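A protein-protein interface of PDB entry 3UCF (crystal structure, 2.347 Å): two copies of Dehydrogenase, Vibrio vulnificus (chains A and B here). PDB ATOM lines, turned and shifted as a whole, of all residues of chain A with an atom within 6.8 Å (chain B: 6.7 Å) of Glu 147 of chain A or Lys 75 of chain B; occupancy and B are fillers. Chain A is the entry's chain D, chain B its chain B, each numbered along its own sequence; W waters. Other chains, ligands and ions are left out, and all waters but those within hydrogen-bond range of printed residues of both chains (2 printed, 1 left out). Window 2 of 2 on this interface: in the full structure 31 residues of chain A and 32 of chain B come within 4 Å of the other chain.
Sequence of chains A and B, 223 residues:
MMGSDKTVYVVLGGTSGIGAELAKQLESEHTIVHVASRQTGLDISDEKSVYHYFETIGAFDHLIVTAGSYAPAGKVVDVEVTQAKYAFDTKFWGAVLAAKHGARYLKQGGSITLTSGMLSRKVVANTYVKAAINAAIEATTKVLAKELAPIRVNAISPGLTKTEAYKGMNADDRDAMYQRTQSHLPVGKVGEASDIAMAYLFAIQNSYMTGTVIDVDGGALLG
Water W1 lies within hydrogen-bond range of OE1 of Glu 147 of chain A (2.8 Å), N of Val 76 of chain B (3.3 Å) and N of Val 77 of chain B (3.4 Å).
Water W2 bridges NZ of Lys 146 of chain A (2.9 Å) and N of Ala 125 of chain B (3.2 Å).
N of Val 76 of chain B lies within hydrogen-bond range of OE1 of Glu 147 of chain A (3.1 Å).
OE2 of Glu 147 of chain A lies within hydrogen-bond range of N of Asn 126 of chain B, 2.7 Å away.
O of Val 79 of chain B is in hydrogen-bond range of NZ of Lys 100 of chain A (3.0 Å).
The side-chain amide oxygen (OD1) of Asn 126 of chain B sits close to the side-chain amino group (NZ) of Lys 75 of chain B.
The backbone carbonyl oxygen (O) of Asn 126 of chain B is in hydrogen-bond range of the backbone NH (N) of Gly 74 of chain B, 2.9 Å away.
Lys 100 of chain A touches Val 76 of chain B (CG to O, 3.7 Å).
Lys 100 of chain A touches Val 77 of chain B.
Val 143 of chain A touches Tyr 128 of chain B.
Leu 144 of chain A touches Val 76 of chain B.
Gly 74 of chain B touches Glu 147 of chain A.
OE1 of Glu 147 of chain A touches CA of Lys 75 of chain B (3.4 Å).
OE2 of Glu 147 of chain A touches C of Ala 125 of chain B, 3.7 Å away.
Of the printed residues of chain B, Lys 100 of chain A touches Val 76 (3.7 Å), Val 77 (3.4 Å) and Val 79 (3.0 Å).
Lys 146 of chain A touches none of the printed residues of chain B.
Of the printed residues of chain B, Glu 147 of chain A touches Gly 74, Lys 75, Val 76, Ala 125 and Asn 126.
Of chain A, only Glu 147 comes within 4 Å of Lys 75 of chain B.
Printed residues of chain A within 4 Å of Val 76 of chain B: Lys 100, Leu 144 and Glu 147.
Printed residues of chain A within 4 Å of Val 77 of chain B: Lys 100.
The nearest printed residue of chain A that does not touch Ala 125 of chain B is Lys 146 of chain A (4.4 Å).
Of the 11 printed residues of chain A, 4 touch a printed residue of chain B.
Hydrophobic or aromatic side chains of chain A within 4 Å of the printed part of chain B: Val 143 and Leu 144.
Along chain A the printed residues that touch a printed residue of chain B span positions 100 to 147.
Of the 13 printed residues of chain B, 8 touch a printed residue of chain A.
Hydrophobic or aromatic side chains of chain B that line the printed part of chain A: Val 76, Val 77, Ala 125 and Tyr 128.
Among the printed residues, no Asp or Glu carboxylate lies within 4 Å of a Lys or Arg side-chain nitrogen of the other chain.
No position is printed for both chains.
Of the 10 pairs that touch across the chains among the printed residues, none has its exchanged pair printed and touching as well.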
ATOM      1  N   LYS A 100     -20.931 -19.759  28.510  1.00  0.00           N
ATOM      2  CA  LYS A 100     -19.590 -19.840  29.084  1.00  0.00           C
ATOM      3  C   LYS A 100     -19.452 -19.005  30.354  1.00  0.00           C
ATOM      4  O   LYS A 100     -18.908 -19.468  31.359  1.00  0.00           O
ATOM      5  CB  LYS A 100     -18.534 -19.394  28.067  1.00  0.00           C
ATOM      6  CG  LYS A 100     -17.125 -19.335  28.653  1.00  0.00           C
ATOM      7  CD  LYS A 100     -16.057 -19.073  27.601  1.00  0.00           C
ATOM      8  CE  LYS A 100     -14.664 -19.296  28.177  1.00  0.00           C
ATOM      9  NZ  LYS A 100     -13.579 -18.870  27.250  1.00  0.00           N
ATOM     10  N   LYS A 142     -26.828 -29.829  23.648  1.00  0.00           N
ATOM     11  CA  LYS A 142     -26.813 -31.170  24.222  1.00  0.00           C
ATOM     12  C   LYS A 142     -25.494 -31.491  24.921  1.00  0.00           C
ATOM     13  O   LYS A 142     -25.482 -32.203  25.925  1.00  0.00           O
ATOM     14  CB  LYS A 142     -27.119 -32.205  23.136  1.00  0.00           C
ATOM     15  CG  LYS A 142     -28.480 -31.986  22.489  1.00  0.00           C
ATOM     16  CD  LYS A 142     -28.879 -33.087  21.520  1.00  0.00           C
ATOM     17  CE  LYS A 142     -30.197 -32.730  20.843  1.00  0.00           C
ATOM     18  NZ  LYS A 142     -30.599 -33.662  19.754  1.00  0.00           N
ATOM     19  N   VAL A 143     -24.388 -30.973  24.395  1.00  0.00           N
ATOM     20  CA  VAL A 143     -23.099 -31.121  25.065  1.00  0.00           C
ATOM     21  C   VAL A 143     -23.119 -30.349  26.383  1.00  0.00           C
ATOM     22  O   VAL A 143     -22.613 -30.825  27.399  1.00  0.00           O
ATOM     23  CB  VAL A 143     -21.930 -30.615  24.196  1.00  0.00           C
ATOM     24  CG1 VAL A 143     -20.625 -30.629  24.989  1.00  0.00           C
ATOM     25  CG2 VAL A 143     -21.796 -31.460  22.941  1.00  0.00           C
ATOM     26  N   LEU A 144     -23.708 -29.158  26.356  1.00  0.00           N
ATOM     27  CA  LEU A 144     -23.826 -28.332  27.555  1.00  0.00           C
ATOM     28  C   LEU A 144     -24.692 -29.015  28.604  1.00  0.00           C
ATOM     29  O   LEU A 144     -24.350 -29.036  29.786  1.00  0.00           O
ATOM     30  CB  LEU A 144     -24.422 -26.964  27.212  1.00  0.00           C
ATOM     31  CG  LEU A 144     -23.439 -25.891  26.742  1.00  0.00           C
ATOM     32  CD1 LEU A 144     -24.183 -24.670  26.219  1.00  0.00           C
ATOM     33  CD2 LEU A 144     -22.492 -25.500  27.867  1.00  0.00           C
ATOM     34  N   ALA A 145     -25.820 -29.568  28.168  1.00  0.00           N
ATOM     35  CA  ALA A 145     -26.733 -30.261  29.069  1.00  0.00           C
ATOM     36  C   ALA A 145     -25.986 -31.358  29.820  1.00  0.00           C
ATOM     37  O   ALA A 145     -26.294 -31.667  30.970  1.00  0.00           O
ATOM     38  CB  ALA A 145     -27.894 -30.853  28.285  1.00  0.00           C
ATOM     39  N   LYS A 146     -24.994 -31.935  29.153  1.00  0.00           N
ATOM     40  CA  LYS A 146     -24.224 -33.038  29.709  1.00  0.00           C
ATOM     41  C   LYS A 146     -23.120 -32.532  30.632  1.00  0.00           C
ATOM     42  O   LYS A 146     -22.940 -33.039  31.739  1.00  0.00           O
ATOM     43  CB  LYS A 146     -23.619 -33.867  28.575  1.00  0.00           C
ATOM     44  CG  LYS A 146     -22.986 -35.176  29.014  1.00  0.00           C
ATOM     45  CD  LYS A 146     -22.883 -36.150  27.849  1.00  0.00           C
ATOM     46  CE  LYS A 146     -22.719 -37.587  28.321  1.00  0.00           C
ATOM     47  NZ  LYS A 146     -22.459 -38.519  27.186  1.00  0.00           N
ATOM     48  N   GLU A 147     -22.385 -31.526  30.170  1.00  0.00           N
ATOM     49  CA  GLU A 147     -21.270 -30.976  30.932  1.00  0.00           C
ATOM     50  C   GLU A 147     -21.738 -30.227  32.176  1.00  0.00           C
ATOM     51  O   GLU A 147     -21.096 -30.293  33.225  1.00  0.00           O
ATOM     52  CB  GLU A 147     -20.435 -30.038  30.054  1.00  0.00           C
ATOM     53  CG  GLU A 147     -19.680 -30.738  28.934  1.00  0.00           C
ATOM     54  CD  GLU A 147     -18.857 -29.774  28.101  1.00  0.00           C
ATOM     55  OE1 GLU A 147     -19.012 -28.548  28.282  1.00  0.00           O
ATOM     56  OE2 GLU A 147     -18.052 -30.242  27.268  1.00  0.00           O
ATOM     57  N   LEU A 148     -22.861 -29.522  32.064  1.00  0.00           N
ATOM     58  CA  LEU A 148     -23.305 -28.624  33.128  1.00  0.00           C
ATOM     59  C   LEU A 148     -24.264 -29.268  34.128  1.00  0.00           C
ATOM     60  O   LEU A 148     -24.578 -28.666  35.155  1.00  0.00           O
ATOM     61  CB  LEU A 148     -23.966 -27.378  32.535  1.00  0.00           C
ATOM     62  CG  LEU A 148     -23.066 -26.420  31.755  1.00  0.00           C
ATOM     63  CD1 LEU A 148     -23.870 -25.210  31.311  1.00  0.00           C
ATOM     64  CD2 LEU A 148     -21.866 -25.983  32.583  1.00  0.00           C
ATOM     65  N   ALA A 149     -24.737 -30.475  33.830  1.00  0.00           N
ATOM     66  CA  ALA A 149     -25.646 -31.171  34.735  1.00  0.00           C
ATOM     67  C   ALA A 149     -25.169 -30.974  36.173  1.00  0.00           C
ATOM     68  O   ALA A 149     -23.964 -30.972  36.428  1.00  0.00           O
ATOM     69  CB  ALA A 149     -25.707 -32.650  34.386  1.00  0.00           C
ATOM     70  N   PRO A 150     -26.104 -30.811  37.126  1.00  0.00           N
ATOM     71  CA  PRO A 150     -27.565 -30.895  37.003  1.00  0.00           C
ATOM     72  C   PRO A 150     -28.240 -29.624  36.481  1.00  0.00           C
ATOM     73  O   PRO A 150     -29.470 -29.579  36.433  1.00  0.00           O
ATOM     74  CB  PRO A 150     -28.011 -31.177  38.439  1.00  0.00           C
ATOM     75  CG  PRO A 150     -26.987 -30.500  39.279  1.00  0.00           C
ATOM     76  CD  PRO A 150     -25.687 -30.584  38.521  1.00  0.00           C
ATOM     77  N   ILE A 151     -27.466 -28.612  36.105  1.00  0.00           N
ATOM     78  CA  ILE A 151     -28.043 -27.453  35.438  1.00  0.00           C
ATOM     79  C   ILE A 151     -28.655 -27.928  34.128  1.00  0.00           C
ATOM     80  O   ILE A 151     -27.990 -28.591  33.332  1.00  0.00           O
ATOM     81  CB  ILE A 151     -26.996 -26.369  35.125  1.00  0.00           C
ATOM     82  CG1 ILE A 151     -26.403 -25.795  36.414  1.00  0.00           C
ATOM     83  CG2 ILE A 151     -27.623 -25.260  34.287  1.00  0.00           C
ATOM     84  CD1 ILE A 151     -27.415 -25.128  37.314  1.00  0.00           C
ATOM     85  N   ALA B  73     -10.053 -29.378  22.494  1.00  0.00           N
ATOM     86  CA  ALA B  73     -10.918 -30.169  23.360  1.00  0.00           C
ATOM     87  C   ALA B  73     -11.175 -29.414  24.662  1.00  0.00           C
ATOM     88  O   ALA B  73     -10.411 -28.521  25.025  1.00  0.00           O
ATOM     89  CB  ALA B  73     -10.273 -31.517  23.650  1.00  0.00           C
ATOM     90  N   GLY B  74     -12.253 -29.764  25.361  1.00  0.00           N
ATOM     91  CA  GLY B  74     -12.532 -29.177  26.663  1.00  0.00           C
ATOM     92  C   GLY B  74     -13.964 -28.712  26.860  1.00  0.00           C
ATOM     93  O   GLY B  74     -14.742 -28.632  25.909  1.00  0.00           O
ATOM     94  N   LYS B  75     -14.310 -28.405  28.109  1.00  0.00           N
ATOM     95  CA  LYS B  75     -15.631 -27.884  28.449  1.00  0.00           C
ATOM     96  C   LYS B  75     -15.882 -26.543  27.762  1.00  0.00           C
ATOM     97  O   LYS B  75     -14.943 -25.815  27.442  1.00  0.00           O
ATOM     98  CB  LYS B  75     -15.758 -27.708  29.968  1.00  0.00           C
ATOM     99  CG  LYS B  75     -16.545 -28.802  30.683  1.00  0.00           C
ATOM    100  CD  LYS B  75     -15.813 -30.131  30.660  1.00  0.00           C
ATOM    101  CE  LYS B  75     -16.411 -31.124  31.650  1.00  0.00           C
ATOM    102  NZ  LYS B  75     -15.734 -32.452  31.600  1.00  0.00           N
ATOM    103  N   VAL B  76     -17.154 -26.221  27.541  1.00  0.00           N
ATOM    104  CA  VAL B  76     -17.531 -24.939  26.954  1.00  0.00           C
ATOM    105  C   VAL B  76     -17.035 -23.779  27.817  1.00  0.00           C
ATOM    106  O   VAL B  76     -16.587 -22.755  27.302  1.00  0.00           O
ATOM    107  CB  VAL B  76     -19.063 -24.820  26.787  1.00  0.00           C
ATOM    108  CG1 VAL B  76     -19.452 -23.404  26.378  1.00  0.00           C
ATOM    109  CG2 VAL B  76     -19.575 -25.825  25.766  1.00  0.00           C
ATOM    110  N   VAL B  77     -17.116 -23.948  29.134  1.00  0.00           N
ATOM    111  CA  VAL B  77     -16.719 -22.897  30.065  1.00  0.00           C
ATOM    112  C   VAL B  77     -15.205 -22.710  30.109  1.00  0.00           C
ATOM    113  O   VAL B  77     -14.720 -21.676  30.565  1.00  0.00           O
ATOM    114  CB  VAL B  77     -17.214 -23.187  31.500  1.00  0.00           C
ATOM    115  CG1 VAL B  77     -18.731 -23.292  31.531  1.00  0.00           C
ATOM    116  CG2 VAL B  77     -16.577 -24.457  32.048  1.00  0.00           C
ATOM    117  N   ASP B  78     -14.465 -23.704  29.628  1.00  0.00           N
ATOM    118  CA  ASP B  78     -13.008 -23.677  29.708  1.00  0.00           C
ATOM    119  C   ASP B  78     -12.352 -23.304  28.380  1.00  0.00           C
ATOM    120  O   ASP B  78     -11.385 -22.542  28.354  1.00  0.00           O
ATOM    121  CB  ASP B  78     -12.483 -25.038  30.168  1.00  0.00           C
ATOM    122  CG  ASP B  78     -12.929 -25.391  31.573  1.00  0.00           C
ATOM    123  OD1 ASP B  78     -13.217 -24.462  32.357  1.00  0.00           O
ATOM    124  OD2 ASP B  78     -12.987 -26.595  31.896  1.00  0.00           O
ATOM    125  N   VAL B  79     -12.879 -23.841  27.284  1.00  0.00           N
ATOM    126  CA  VAL B  79     -12.272 -23.653  25.970  1.00  0.00           C
ATOM    127  C   VAL B  79     -12.176 -22.181  25.581  1.00  0.00           C
ATOM    128  O   VAL B  79     -13.148 -21.432  25.691  1.00  0.00           O
ATOM    129  CB  VAL B  79     -13.061 -24.403  24.877  1.00  0.00           C
ATOM    130  CG1 VAL B  79     -12.610 -23.960  23.490  1.00  0.00           C
ATOM    131  CG2 VAL B  79     -12.899 -25.906  25.042  1.00  0.00           C
ATOM    132  N   GLU B  80     -10.994 -21.780  25.122  1.00  0.00           N
ATOM    133  CA  GLU B  80     -10.775 -20.427  24.627  1.00  0.00           C
ATOM    134  C   GLU B  80     -11.505 -20.249  23.299  1.00  0.00           C
ATOM    135  O   GLU B  80     -11.247 -20.971  22.336  1.00  0.00           O
ATOM    136  CB  GLU B  80      -9.280 -20.159  24.448  1.00  0.00           C
ATOM    137  N   VAL B 124     -20.766 -36.120  23.509  1.00  0.00           N
ATOM    138  CA  VAL B 124     -19.599 -36.440  24.322  1.00  0.00           C
ATOM    139  C   VAL B 124     -19.037 -35.186  24.975  1.00  0.00           C
ATOM    140  O   VAL B 124     -18.744 -34.202  24.296  1.00  0.00           O
ATOM    141  CB  VAL B 124     -18.489 -37.076  23.466  1.00  0.00           C
ATOM    142  CG1 VAL B 124     -17.225 -37.268  24.287  1.00  0.00           C
ATOM    143  CG2 VAL B 124     -18.960 -38.396  22.886  1.00  0.00           C
ATOM    144  N   ALA B 125     -18.878 -35.226  26.293  1.00  0.00           N
ATOM    145  CA  ALA B 125     -18.346 -34.087  27.031  1.00  0.00           C
ATOM    146  C   ALA B 125     -16.980 -33.691  26.480  1.00  0.00           C
ATOM    147  O   ALA B 125     -16.193 -34.550  26.086  1.00  0.00           O
ATOM    148  CB  ALA B 125     -18.247 -34.418  28.515  1.00  0.00           C
ATOM    149  N   ASN B 126     -16.717 -32.386  26.441  1.00  0.00           N
ATOM    150  CA  ASN B 126     -15.423 -31.852  26.010  1.00  0.00           C
ATOM    151  C   ASN B 126     -15.257 -31.750  24.491  1.00  0.00           C
ATOM    152  O   ASN B 126     -14.166 -31.439  24.013  1.00  0.00           O
ATOM    153  CB  ASN B 126     -14.267 -32.681  26.590  1.00  0.00           C
ATOM    154  CG  ASN B 126     -14.243 -32.672  28.105  1.00  0.00           C
ATOM    155  OD1 ASN B 126     -14.498 -31.646  28.728  1.00  0.00           O
ATOM    156  ND2 ASN B 126     -13.933 -33.817  28.708  1.00  0.00           N
ATOM    157  N   THR B 127     -16.322 -31.997  23.731  1.00  0.00           N
ATOM    158  CA  THR B 127     -16.209 -32.026  22.270  1.00  0.00           C
ATOM    159  C   THR B 127     -17.174 -31.079  21.555  1.00  0.00           C
ATOM    160  O   THR B 127     -17.575 -31.343  20.421  1.00  0.00           O
ATOM    161  CB  THR B 127     -16.463 -33.443  21.713  1.00  0.00           C
ATOM    162  OG1 THR B 127     -17.836 -33.805  21.914  1.00  0.00           O
ATOM    163  CG2 THR B 127     -15.560 -34.462  22.385  1.00  0.00           C
ATOM    164  N   TYR B 128     -17.533 -29.973  22.199  1.00  0.00           N
ATOM    165  CA  TYR B 128     -18.555 -29.082  21.651  1.00  0.00           C
ATOM    166  C   TYR B 128     -18.107 -28.380  20.367  1.00  0.00           C
ATOM    167  O   TYR B 128     -18.937 -28.034  19.527  1.00  0.00           O
ATOM    168  CB  TYR B 128     -19.004 -28.052  22.694  1.00  0.00           C
ATOM    169  CG  TYR B 128     -18.344 -26.697  22.571  1.00  0.00           C
ATOM    170  CD1 TYR B 128     -18.804 -25.763  21.651  1.00  0.00           C
ATOM    171  CD2 TYR B 128     -17.274 -26.342  23.385  1.00  0.00           C
ATOM    172  CE1 TYR B 128     -18.213 -24.520  21.536  1.00  0.00           C
ATOM    173  CE2 TYR B 128     -16.675 -25.098  23.278  1.00  0.00           C
ATOM    174  CZ  TYR B 128     -17.148 -24.191  22.351  1.00  0.00           C
ATOM    175  OH  TYR B 128     -16.551 -22.956  22.245  1.00  0.00           O
HETATM  176  O   HOH W   1     -19.198 -26.415  30.070  1.00  0.00           O
HETATM  177  O   HOH W   2     -19.676 -37.899  27.920  1.00  0.00           O
